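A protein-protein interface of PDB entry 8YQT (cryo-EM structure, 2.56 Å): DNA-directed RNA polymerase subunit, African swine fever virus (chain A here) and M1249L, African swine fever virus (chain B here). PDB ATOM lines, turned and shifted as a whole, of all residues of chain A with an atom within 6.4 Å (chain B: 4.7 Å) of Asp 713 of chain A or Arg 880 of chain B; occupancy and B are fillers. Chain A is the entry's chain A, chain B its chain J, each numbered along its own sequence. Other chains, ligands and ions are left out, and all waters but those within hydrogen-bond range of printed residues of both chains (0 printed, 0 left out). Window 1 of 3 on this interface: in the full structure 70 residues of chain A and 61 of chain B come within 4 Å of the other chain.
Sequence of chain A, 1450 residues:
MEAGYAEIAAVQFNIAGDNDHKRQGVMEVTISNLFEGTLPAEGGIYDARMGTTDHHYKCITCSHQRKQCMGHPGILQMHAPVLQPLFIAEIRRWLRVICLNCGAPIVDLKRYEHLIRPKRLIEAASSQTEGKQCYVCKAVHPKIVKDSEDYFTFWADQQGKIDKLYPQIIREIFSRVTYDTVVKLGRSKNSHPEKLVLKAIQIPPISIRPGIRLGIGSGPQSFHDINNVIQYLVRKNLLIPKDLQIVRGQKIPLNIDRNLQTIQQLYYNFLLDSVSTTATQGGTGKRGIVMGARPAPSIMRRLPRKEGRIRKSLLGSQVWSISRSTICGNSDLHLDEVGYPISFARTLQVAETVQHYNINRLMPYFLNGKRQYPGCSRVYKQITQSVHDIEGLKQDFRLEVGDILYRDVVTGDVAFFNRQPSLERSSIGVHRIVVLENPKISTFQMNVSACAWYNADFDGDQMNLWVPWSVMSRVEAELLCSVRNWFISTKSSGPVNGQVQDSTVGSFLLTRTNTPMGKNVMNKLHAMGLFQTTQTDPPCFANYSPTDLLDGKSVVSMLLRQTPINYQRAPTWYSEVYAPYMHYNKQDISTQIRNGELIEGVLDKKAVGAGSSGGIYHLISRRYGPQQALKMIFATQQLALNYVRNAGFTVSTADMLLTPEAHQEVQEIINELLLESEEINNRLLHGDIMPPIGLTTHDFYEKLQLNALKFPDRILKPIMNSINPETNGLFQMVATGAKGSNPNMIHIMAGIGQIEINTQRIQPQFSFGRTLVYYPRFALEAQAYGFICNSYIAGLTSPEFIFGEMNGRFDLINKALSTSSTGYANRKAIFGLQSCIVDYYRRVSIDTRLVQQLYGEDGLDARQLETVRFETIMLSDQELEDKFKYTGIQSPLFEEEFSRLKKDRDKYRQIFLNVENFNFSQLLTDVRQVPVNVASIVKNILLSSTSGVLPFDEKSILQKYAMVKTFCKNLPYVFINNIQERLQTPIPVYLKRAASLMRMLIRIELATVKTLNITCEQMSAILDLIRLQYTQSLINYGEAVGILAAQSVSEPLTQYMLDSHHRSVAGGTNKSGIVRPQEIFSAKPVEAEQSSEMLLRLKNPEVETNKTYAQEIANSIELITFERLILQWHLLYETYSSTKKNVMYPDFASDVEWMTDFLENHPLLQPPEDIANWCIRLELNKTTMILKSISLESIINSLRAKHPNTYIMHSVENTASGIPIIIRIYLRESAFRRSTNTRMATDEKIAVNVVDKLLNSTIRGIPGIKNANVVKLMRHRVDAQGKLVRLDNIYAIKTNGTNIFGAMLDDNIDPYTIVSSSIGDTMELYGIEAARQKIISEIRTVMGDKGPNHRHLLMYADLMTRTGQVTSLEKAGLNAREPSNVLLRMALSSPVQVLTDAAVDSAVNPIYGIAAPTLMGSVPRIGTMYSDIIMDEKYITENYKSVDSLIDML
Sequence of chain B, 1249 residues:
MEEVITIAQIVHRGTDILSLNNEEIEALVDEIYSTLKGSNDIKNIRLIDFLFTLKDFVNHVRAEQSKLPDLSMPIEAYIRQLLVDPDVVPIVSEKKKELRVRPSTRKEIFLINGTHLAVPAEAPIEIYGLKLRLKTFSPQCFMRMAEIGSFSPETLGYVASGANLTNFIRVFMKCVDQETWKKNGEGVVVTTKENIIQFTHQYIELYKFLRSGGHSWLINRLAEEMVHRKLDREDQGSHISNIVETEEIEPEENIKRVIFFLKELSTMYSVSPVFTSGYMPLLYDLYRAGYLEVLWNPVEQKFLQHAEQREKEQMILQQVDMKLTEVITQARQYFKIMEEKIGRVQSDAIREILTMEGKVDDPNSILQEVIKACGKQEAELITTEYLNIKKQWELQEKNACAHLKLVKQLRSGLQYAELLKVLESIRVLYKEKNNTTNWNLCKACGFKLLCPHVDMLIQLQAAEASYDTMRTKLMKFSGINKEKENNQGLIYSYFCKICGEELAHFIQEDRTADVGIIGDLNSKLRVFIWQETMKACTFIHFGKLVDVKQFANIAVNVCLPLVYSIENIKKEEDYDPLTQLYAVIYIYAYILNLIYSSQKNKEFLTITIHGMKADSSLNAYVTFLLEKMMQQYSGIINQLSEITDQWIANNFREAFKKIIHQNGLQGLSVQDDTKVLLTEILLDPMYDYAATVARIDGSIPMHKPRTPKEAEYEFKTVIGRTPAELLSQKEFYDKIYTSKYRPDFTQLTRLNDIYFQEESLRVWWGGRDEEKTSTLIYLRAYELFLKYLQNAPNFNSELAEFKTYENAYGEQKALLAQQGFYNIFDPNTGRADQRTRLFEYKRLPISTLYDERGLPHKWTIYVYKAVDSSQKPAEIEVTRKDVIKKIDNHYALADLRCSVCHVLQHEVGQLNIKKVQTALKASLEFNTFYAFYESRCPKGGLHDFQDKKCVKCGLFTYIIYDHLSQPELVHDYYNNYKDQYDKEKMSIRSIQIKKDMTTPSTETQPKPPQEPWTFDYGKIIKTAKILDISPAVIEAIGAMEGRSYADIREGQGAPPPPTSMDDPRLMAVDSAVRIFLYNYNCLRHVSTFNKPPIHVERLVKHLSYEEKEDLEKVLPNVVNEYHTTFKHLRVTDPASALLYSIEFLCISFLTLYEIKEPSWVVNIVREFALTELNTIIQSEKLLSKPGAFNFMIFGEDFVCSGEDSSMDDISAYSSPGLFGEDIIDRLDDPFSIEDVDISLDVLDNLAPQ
OD2 of Asp 713 of chain A is in salt-bridge range of NH1 of Arg 880 of chain B (3.3 Å).
The backbone carbonyl oxygen of Val 878 of chain B lies within hydrogen-bond range of the backbone NH of Tyr 862 of chain B, at 2.9 Å.
The side-chain carboxylate of Glu 576 of chain A is in hydrogen-bond range of the side-chain hydroxyl of Tyr 574 of chain A (3.2 Å).
Glu 576 of chain A touches Arg 880 of chain B (O to NE, 3.5 Å).
CG of Lys 881 of chain B touches OE1 of Glu 576 of chain A, at 3.4 Å.
Ala 579 of chain A touches Val 883 of chain B.
Pro 580 of chain A touches Tyr 862 of chain B (CB to CE1, 3.5 Å).
Pro 580 of chain A touches Arg 880 of chain B.
Pro 580 of chain A touches Val 883 of chain B.
Tyr 581 of chain A touches Tyr 862 of chain B (OH to OH, 3.6 Å).
Of chain B, only Arg 880 (3.3 Å) comes within 4 Å of Asp 713 of chain A.
Arg 880 of chain B touches just these residues of chain A: Glu 576, Pro 580 and Asp 713.
Printed residues of chain B within 4 Å of Pro 580 of chain A: Tyr 862 (3.5 Å), Arg 880 (3.5 Å) and Val 883 (3.9 Å).
Of the printed residues of chain B, Ala 579 of chain A touches Val 883.
Of the printed residues of chain B, Glu 576 of chain A touches Arg 880 and Lys 881.
Leu 716 of chain A touches none of the printed residues of chain B.
The nearest residue of chain A that does not touch Arg 880 of chain B is Val 577 of chain A (4.1 Å).
The nearest printed residue of chain B that does not touch Glu 576 of chain A is Asp 882 of chain B (5.9 Å).
Hydrophobic or aromatic side chains of chain B within 4 Å of the printed part of chain A: Tyr 862 and Val 883.
Printed residues of chain A that touch a printed residue of chain B: Glu 576, Ala 579, Pro 580, Tyr 581 and Asp 713.
Along chain A the printed residues that touch a printed residue of chain B span positions 576 to 713.
Among the printed residues, Asp or Glu carboxylates within 4 Å of a Lys or Arg side-chain nitrogen of the other chain: Asp 713 of chain A with Arg 880 of chain B (3.3 Å).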
ATOM      1  N   TYR A 574      -1.346  -9.637  11.106  1.00  0.00           N
ATOM      2  CA  TYR A 574      -0.714  -8.583  11.887  1.00  0.00           C
ATOM      3  C   TYR A 574      -0.325  -7.431  10.972  1.00  0.00           C
ATOM      4  O   TYR A 574       0.527  -7.583  10.095  1.00  0.00           O
ATOM      5  CB  TYR A 574       0.512  -9.087  12.637  1.00  0.00           C
ATOM      6  CG  TYR A 574       1.241  -7.938  13.284  1.00  0.00           C
ATOM      7  CD1 TYR A 574       0.692  -7.277  14.371  1.00  0.00           C
ATOM      8  CD2 TYR A 574       2.449  -7.482  12.782  1.00  0.00           C
ATOM      9  CE1 TYR A 574       1.335  -6.214  14.957  1.00  0.00           C
ATOM     10  CE2 TYR A 574       3.103  -6.416  13.363  1.00  0.00           C
ATOM     11  CZ  TYR A 574       2.541  -5.785  14.450  1.00  0.00           C
ATOM     12  OH  TYR A 574       3.185  -4.723  15.036  1.00  0.00           O
ATOM     13  N   GLU A 576       0.809  -3.249  11.365  1.00  0.00           N
ATOM     14  CA  GLU A 576       1.102  -2.134  12.257  1.00  0.00           C
ATOM     15  C   GLU A 576       0.072  -1.023  12.123  1.00  0.00           C
ATOM     16  O   GLU A 576      -0.045  -0.185  13.021  1.00  0.00           O
ATOM     17  CB  GLU A 576       2.502  -1.591  11.981  1.00  0.00           C
ATOM     18  CG  GLU A 576       3.109  -0.826  13.139  1.00  0.00           C
ATOM     19  CD  GLU A 576       4.560  -1.190  13.379  1.00  0.00           C
ATOM     20  OE1 GLU A 576       5.417  -0.282  13.329  1.00  0.00           O
ATOM     21  OE2 GLU A 576       4.845  -2.383  13.618  1.00  0.00           O
ATOM     22  N   VAL A 577      -0.675  -1.013  11.021  1.00  0.00           N
ATOM     23  CA  VAL A 577      -1.739  -0.038  10.825  1.00  0.00           C
ATOM     24  C   VAL A 577      -2.887  -0.295  11.794  1.00  0.00           C
ATOM     25  O   VAL A 577      -3.486   0.642  12.333  1.00  0.00           O
ATOM     26  CB  VAL A 577      -2.205  -0.078   9.359  1.00  0.00           C
ATOM     27  CG1 VAL A 577      -3.470   0.697   9.177  1.00  0.00           C
ATOM     28  CG2 VAL A 577      -1.119   0.462   8.452  1.00  0.00           C
ATOM     29  N   ALA A 579      -2.606  -2.133  14.659  1.00  0.00           N
ATOM     30  CA  ALA A 579      -2.161  -2.453  16.010  1.00  0.00           C
ATOM     31  C   ALA A 579      -2.645  -1.486  17.089  1.00  0.00           C
ATOM     32  O   ALA A 579      -3.023  -1.972  18.168  1.00  0.00           O
ATOM     33  CB  ALA A 579      -0.630  -2.555  16.033  1.00  0.00           C
ATOM     34  N   PRO A 580      -2.634  -0.160  16.904  1.00  0.00           N
ATOM     35  CA  PRO A 580      -3.097   0.714  17.991  1.00  0.00           C
ATOM     36  C   PRO A 580      -4.551   0.516  18.373  1.00  0.00           C
ATOM     37  O   PRO A 580      -4.892   0.681  19.549  1.00  0.00           O
ATOM     38  CB  PRO A 580      -2.859   2.122  17.431  1.00  0.00           C
ATOM     39  CG  PRO A 580      -1.824   1.949  16.424  1.00  0.00           C
ATOM     40  CD  PRO A 580      -2.089   0.634  15.791  1.00  0.00           C
ATOM     41  N   TYR A 581      -5.417   0.170  17.424  1.00  0.00           N
ATOM     42  CA  TYR A 581      -6.856   0.206  17.644  1.00  0.00           C
ATOM     43  C   TYR A 581      -7.463  -1.174  17.855  1.00  0.00           C
ATOM     44  O   TYR A 581      -8.691  -1.295  17.914  1.00  0.00           O
ATOM     45  CB  TYR A 581      -7.541   0.908  16.471  1.00  0.00           C
ATOM     46  CG  TYR A 581      -6.792   2.115  15.960  1.00  0.00           C
ATOM     47  CD1 TYR A 581      -6.745   3.287  16.696  1.00  0.00           C
ATOM     48  CD2 TYR A 581      -6.134   2.080  14.744  1.00  0.00           C
ATOM     49  CE1 TYR A 581      -6.064   4.387  16.236  1.00  0.00           C
ATOM     50  CE2 TYR A 581      -5.451   3.175  14.276  1.00  0.00           C
ATOM     51  CZ  TYR A 581      -5.418   4.328  15.026  1.00  0.00           C
ATOM     52  OH  TYR A 581      -4.736   5.425  14.560  1.00  0.00           O
ATOM     53  N   PHE A 711      -6.375  11.837   3.564  1.00  0.00           N
ATOM     54  CA  PHE A 711      -6.807  11.332   4.857  1.00  0.00           C
ATOM     55  C   PHE A 711      -5.594  11.022   5.729  1.00  0.00           C
ATOM     56  O   PHE A 711      -4.600  10.478   5.241  1.00  0.00           O
ATOM     57  CB  PHE A 711      -7.661  10.076   4.699  1.00  0.00           C
ATOM     58  CG  PHE A 711      -9.058  10.348   4.235  1.00  0.00           C
ATOM     59  CD1 PHE A 711      -9.532  11.639   4.141  1.00  0.00           C
ATOM     60  CD2 PHE A 711      -9.904   9.310   3.907  1.00  0.00           C
ATOM     61  CE1 PHE A 711     -10.817  11.892   3.719  1.00  0.00           C
ATOM     62  CE2 PHE A 711     -11.188   9.558   3.488  1.00  0.00           C
ATOM     63  CZ  PHE A 711     -11.644  10.851   3.393  1.00  0.00           C
ATOM     64  N   PRO A 712      -5.638  11.359   7.008  1.00  0.00           N
ATOM     65  CA  PRO A 712      -4.556  10.993   7.921  1.00  0.00           C
ATOM     66  C   PRO A 712      -4.637   9.511   8.272  1.00  0.00           C
ATOM     67  O   PRO A 712      -5.595   8.819   7.941  1.00  0.00           O
ATOM     68  CB  PRO A 712      -4.816  11.881   9.139  1.00  0.00           C
ATOM     69  CG  PRO A 712      -6.271  12.114   9.119  1.00  0.00           C
ATOM     70  CD  PRO A 712      -6.675  12.163   7.675  1.00  0.00           C
ATOM     71  N   ASP A 713      -3.594   9.027   8.946  1.00  0.00           N
ATOM     72  CA  ASP A 713      -3.599   7.642   9.404  1.00  0.00           C
ATOM     73  C   ASP A 713      -4.660   7.410  10.468  1.00  0.00           C
ATOM     74  O   ASP A 713      -5.205   6.306  10.569  1.00  0.00           O
ATOM     75  CB  ASP A 713      -2.221   7.254   9.939  1.00  0.00           C
ATOM     76  CG  ASP A 713      -1.246   6.901   8.836  1.00  0.00           C
ATOM     77  OD1 ASP A 713      -1.701   6.443   7.767  1.00  0.00           O
ATOM     78  OD2 ASP A 713      -0.026   7.074   9.038  1.00  0.00           O
ATOM     79  N   ARG A 714      -4.972   8.435  11.259  1.00  0.00           N
ATOM     80  CA  ARG A 714      -5.931   8.311  12.348  1.00  0.00           C
ATOM     81  C   ARG A 714      -7.373   8.217  11.877  1.00  0.00           C
ATOM     82  O   ARG A 714      -8.270   8.188  12.723  1.00  0.00           O
ATOM     83  CB  ARG A 714      -5.776   9.489  13.306  1.00  0.00           C
ATOM     84  CG  ARG A 714      -6.129  10.827  12.696  1.00  0.00           C
ATOM     85  CD  ARG A 714      -5.541  11.965  13.504  1.00  0.00           C
ATOM     86  NE  ARG A 714      -6.024  13.259  13.044  1.00  0.00           N
ATOM     87  CZ  ARG A 714      -7.176  13.800  13.411  1.00  0.00           C
ATOM     88  NH1 ARG A 714      -8.006  13.171  14.225  1.00  0.00           N
ATOM     89  NH2 ARG A 714      -7.506  15.001  12.944  1.00  0.00           N
ATOM     90  N   ILE A 715      -7.627   8.170  10.568  1.00  0.00           N
ATOM     91  CA  ILE A 715      -8.985   7.956  10.090  1.00  0.00           C
ATOM     92  C   ILE A 715      -9.469   6.558  10.435  1.00  0.00           C
ATOM     93  O   ILE A 715     -10.678   6.306  10.449  1.00  0.00           O
ATOM     94  CB  ILE A 715      -9.071   8.223   8.571  1.00  0.00           C
ATOM     95  CG1 ILE A 715     -10.530   8.347   8.125  1.00  0.00           C
ATOM     96  CG2 ILE A 715      -8.379   7.123   7.795  1.00  0.00           C
ATOM     97  CD1 ILE A 715     -11.251   9.530   8.709  1.00  0.00           C
ATOM     98  N   LEU A 716      -8.553   5.636  10.725  1.00  0.00           N
ATOM     99  CA  LEU A 716      -8.934   4.280  11.089  1.00  0.00           C
ATOM    100  C   LEU A 716      -9.330   4.140  12.550  1.00  0.00           C
ATOM    101  O   LEU A 716      -9.892   3.105  12.918  1.00  0.00           O
ATOM    102  CB  LEU A 716      -7.801   3.309  10.768  1.00  0.00           C
ATOM    103  CG  LEU A 716      -7.912   2.656   9.392  1.00  0.00           C
ATOM    104  CD1 LEU A 716      -6.563   2.209   8.922  1.00  0.00           C
ATOM    105  CD2 LEU A 716      -8.873   1.484   9.423  1.00  0.00           C
ATOM    106  N   LYS A 717      -9.053   5.134  13.390  1.00  0.00           N
ATOM    107  CA  LYS A 717      -9.539   5.073  14.766  1.00  0.00           C
ATOM    108  C   LYS A 717     -11.059   5.033  14.843  1.00  0.00           C
ATOM    109  O   LYS A 717     -11.593   4.154  15.539  1.00  0.00           O
ATOM    110  CB  LYS A 717      -8.961   6.236  15.576  1.00  0.00           C
ATOM    111  CG  LYS A 717      -9.470   6.304  17.001  1.00  0.00           C
ATOM    112  CD  LYS A 717      -8.723   7.351  17.804  1.00  0.00           C
ATOM    113  CE  LYS A 717      -9.229   7.410  19.231  1.00  0.00           C
ATOM    114  NZ  LYS A 717     -10.643   7.863  19.285  1.00  0.00           N
ATOM    115  N   TYR B 862       0.015   7.467  21.334  1.00  0.00           N
ATOM    116  CA  TYR B 862      -1.201   6.772  21.726  1.00  0.00           C
ATOM    117  C   TYR B 862      -1.211   6.612  23.237  1.00  0.00           C
ATOM    118  O   TYR B 862      -0.233   6.132  23.821  1.00  0.00           O
ATOM    119  CB  TYR B 862      -1.292   5.407  21.043  1.00  0.00           C
ATOM    120  CG  TYR B 862      -1.276   5.485  19.536  1.00  0.00           C
ATOM    121  CD1 TYR B 862      -2.455   5.495  18.811  1.00  0.00           C
ATOM    122  CD2 TYR B 862      -0.080   5.557  18.839  1.00  0.00           C
ATOM    123  CE1 TYR B 862      -2.443   5.573  17.435  1.00  0.00           C
ATOM    124  CE2 TYR B 862      -0.060   5.636  17.468  1.00  0.00           C
ATOM    125  CZ  TYR B 862      -1.242   5.642  16.770  1.00  0.00           C
ATOM    126  OH  TYR B 862      -1.223   5.719  15.400  1.00  0.00           O
ATOM    127  N   VAL B 878       2.504   5.155  24.171  1.00  0.00           N
ATOM    128  CA  VAL B 878       3.376   4.459  23.233  1.00  0.00           C
ATOM    129  C   VAL B 878       3.068   4.909  21.813  1.00  0.00           C
ATOM    130  O   VAL B 878       1.981   5.402  21.512  1.00  0.00           O
ATOM    131  CB  VAL B 878       3.243   2.923  23.336  1.00  0.00           C
ATOM    132  CG1 VAL B 878       3.752   2.428  24.679  1.00  0.00           C
ATOM    133  CG2 VAL B 878       1.804   2.493  23.110  1.00  0.00           C
ATOM    134  N   THR B 879       4.042   4.715  20.930  1.00  0.00           N
ATOM    135  CA  THR B 879       3.880   4.979  19.510  1.00  0.00           C
ATOM    136  C   THR B 879       3.512   3.682  18.789  1.00  0.00           C
ATOM    137  O   THR B 879       3.464   2.607  19.387  1.00  0.00           O
ATOM    138  CB  THR B 879       5.151   5.606  18.933  1.00  0.00           C
ATOM    139  OG1 THR B 879       4.943   5.929  17.553  1.00  0.00           O
ATOM    140  CG2 THR B 879       6.323   4.648  19.055  1.00  0.00           C
ATOM    141  N   ARG B 880       3.249   3.788  17.482  1.00  0.00           N
ATOM    142  CA  ARG B 880       2.738   2.642  16.730  1.00  0.00           C
ATOM    143  C   ARG B 880       3.685   1.452  16.771  1.00  0.00           C
ATOM    144  O   ARG B 880       3.233   0.301  16.755  1.00  0.00           O
ATOM    145  CB  ARG B 880       2.471   3.028  15.276  1.00  0.00           C
ATOM    146  CG  ARG B 880       1.023   3.306  14.971  1.00  0.00           C
ATOM    147  CD  ARG B 880       0.842   3.893  13.589  1.00  0.00           C
ATOM    148  NE  ARG B 880       1.332   3.003  12.546  1.00  0.00           N
ATOM    149  CZ  ARG B 880       1.452   3.349  11.272  1.00  0.00           C
ATOM    150  NH1 ARG B 880       1.125   4.559  10.852  1.00  0.00           N
ATOM    151  NH2 ARG B 880       1.912   2.458  10.397  1.00  0.00           N
ATOM    152  N   LYS B 881       4.994   1.701  16.808  1.00  0.00           N
ATOM    153  CA  LYS B 881       5.949   0.600  16.775  1.00  0.00           C
ATOM    154  C   LYS B 881       5.882  -0.248  18.038  1.00  0.00           C
ATOM    155  O   LYS B 881       6.053  -1.470  17.969  1.00  0.00           O
ATOM    156  CB  LYS B 881       7.364   1.141  16.576  1.00  0.00           C
ATOM    157  CG  LYS B 881       7.687   1.534  15.145  1.00  0.00           C
ATOM    158  CD  LYS B 881       8.404   2.873  15.090  1.00  0.00           C
ATOM    159  CE  LYS B 881       7.470   4.024  15.433  1.00  0.00           C
ATOM    160  NZ  LYS B 881       6.928   4.688  14.214  1.00  0.00           N
ATOM    161  N   ASP B 882       5.633   0.370  19.193  1.00  0.00           N
ATOM    162  CA  ASP B 882       5.713  -0.309  20.480  1.00  0.00           C
ATOM    163  C   ASP B 882       4.346  -0.653  21.061  1.00  0.00           C
ATOM    164  O   ASP B 882       4.255  -1.023  22.235  1.00  0.00           O
ATOM    165  CB  ASP B 882       6.507   0.538  21.472  1.00  0.00           C
ATOM    166  CG  ASP B 882       7.789   1.078  20.878  1.00  0.00           C
ATOM    167  OD1 ASP B 882       7.755   1.547  19.722  1.00  0.00           O
ATOM    168  OD2 ASP B 882       8.832   1.034  21.565  1.00  0.00           O
ATOM    169  N   VAL B 883       3.277  -0.528  20.273  1.00  0.00           N
ATOM    170  CA  VAL B 883       1.958  -0.910  20.765  1.00  0.00           C
ATOM    171  C   VAL B 883       1.905  -2.408  21.034  1.00  0.00           C
ATOM    172  O   VAL B 883       1.399  -2.851  22.072  1.00  0.00           O
ATOM    173  CB  VAL B 883       0.866  -0.474  19.773  1.00  0.00           C
ATOM    174  CG1 VAL B 883      -0.460  -1.106  20.141  1.00  0.00           C
ATOM    175  CG2 VAL B 883       0.737   1.036  19.759  1.00  0.00           C
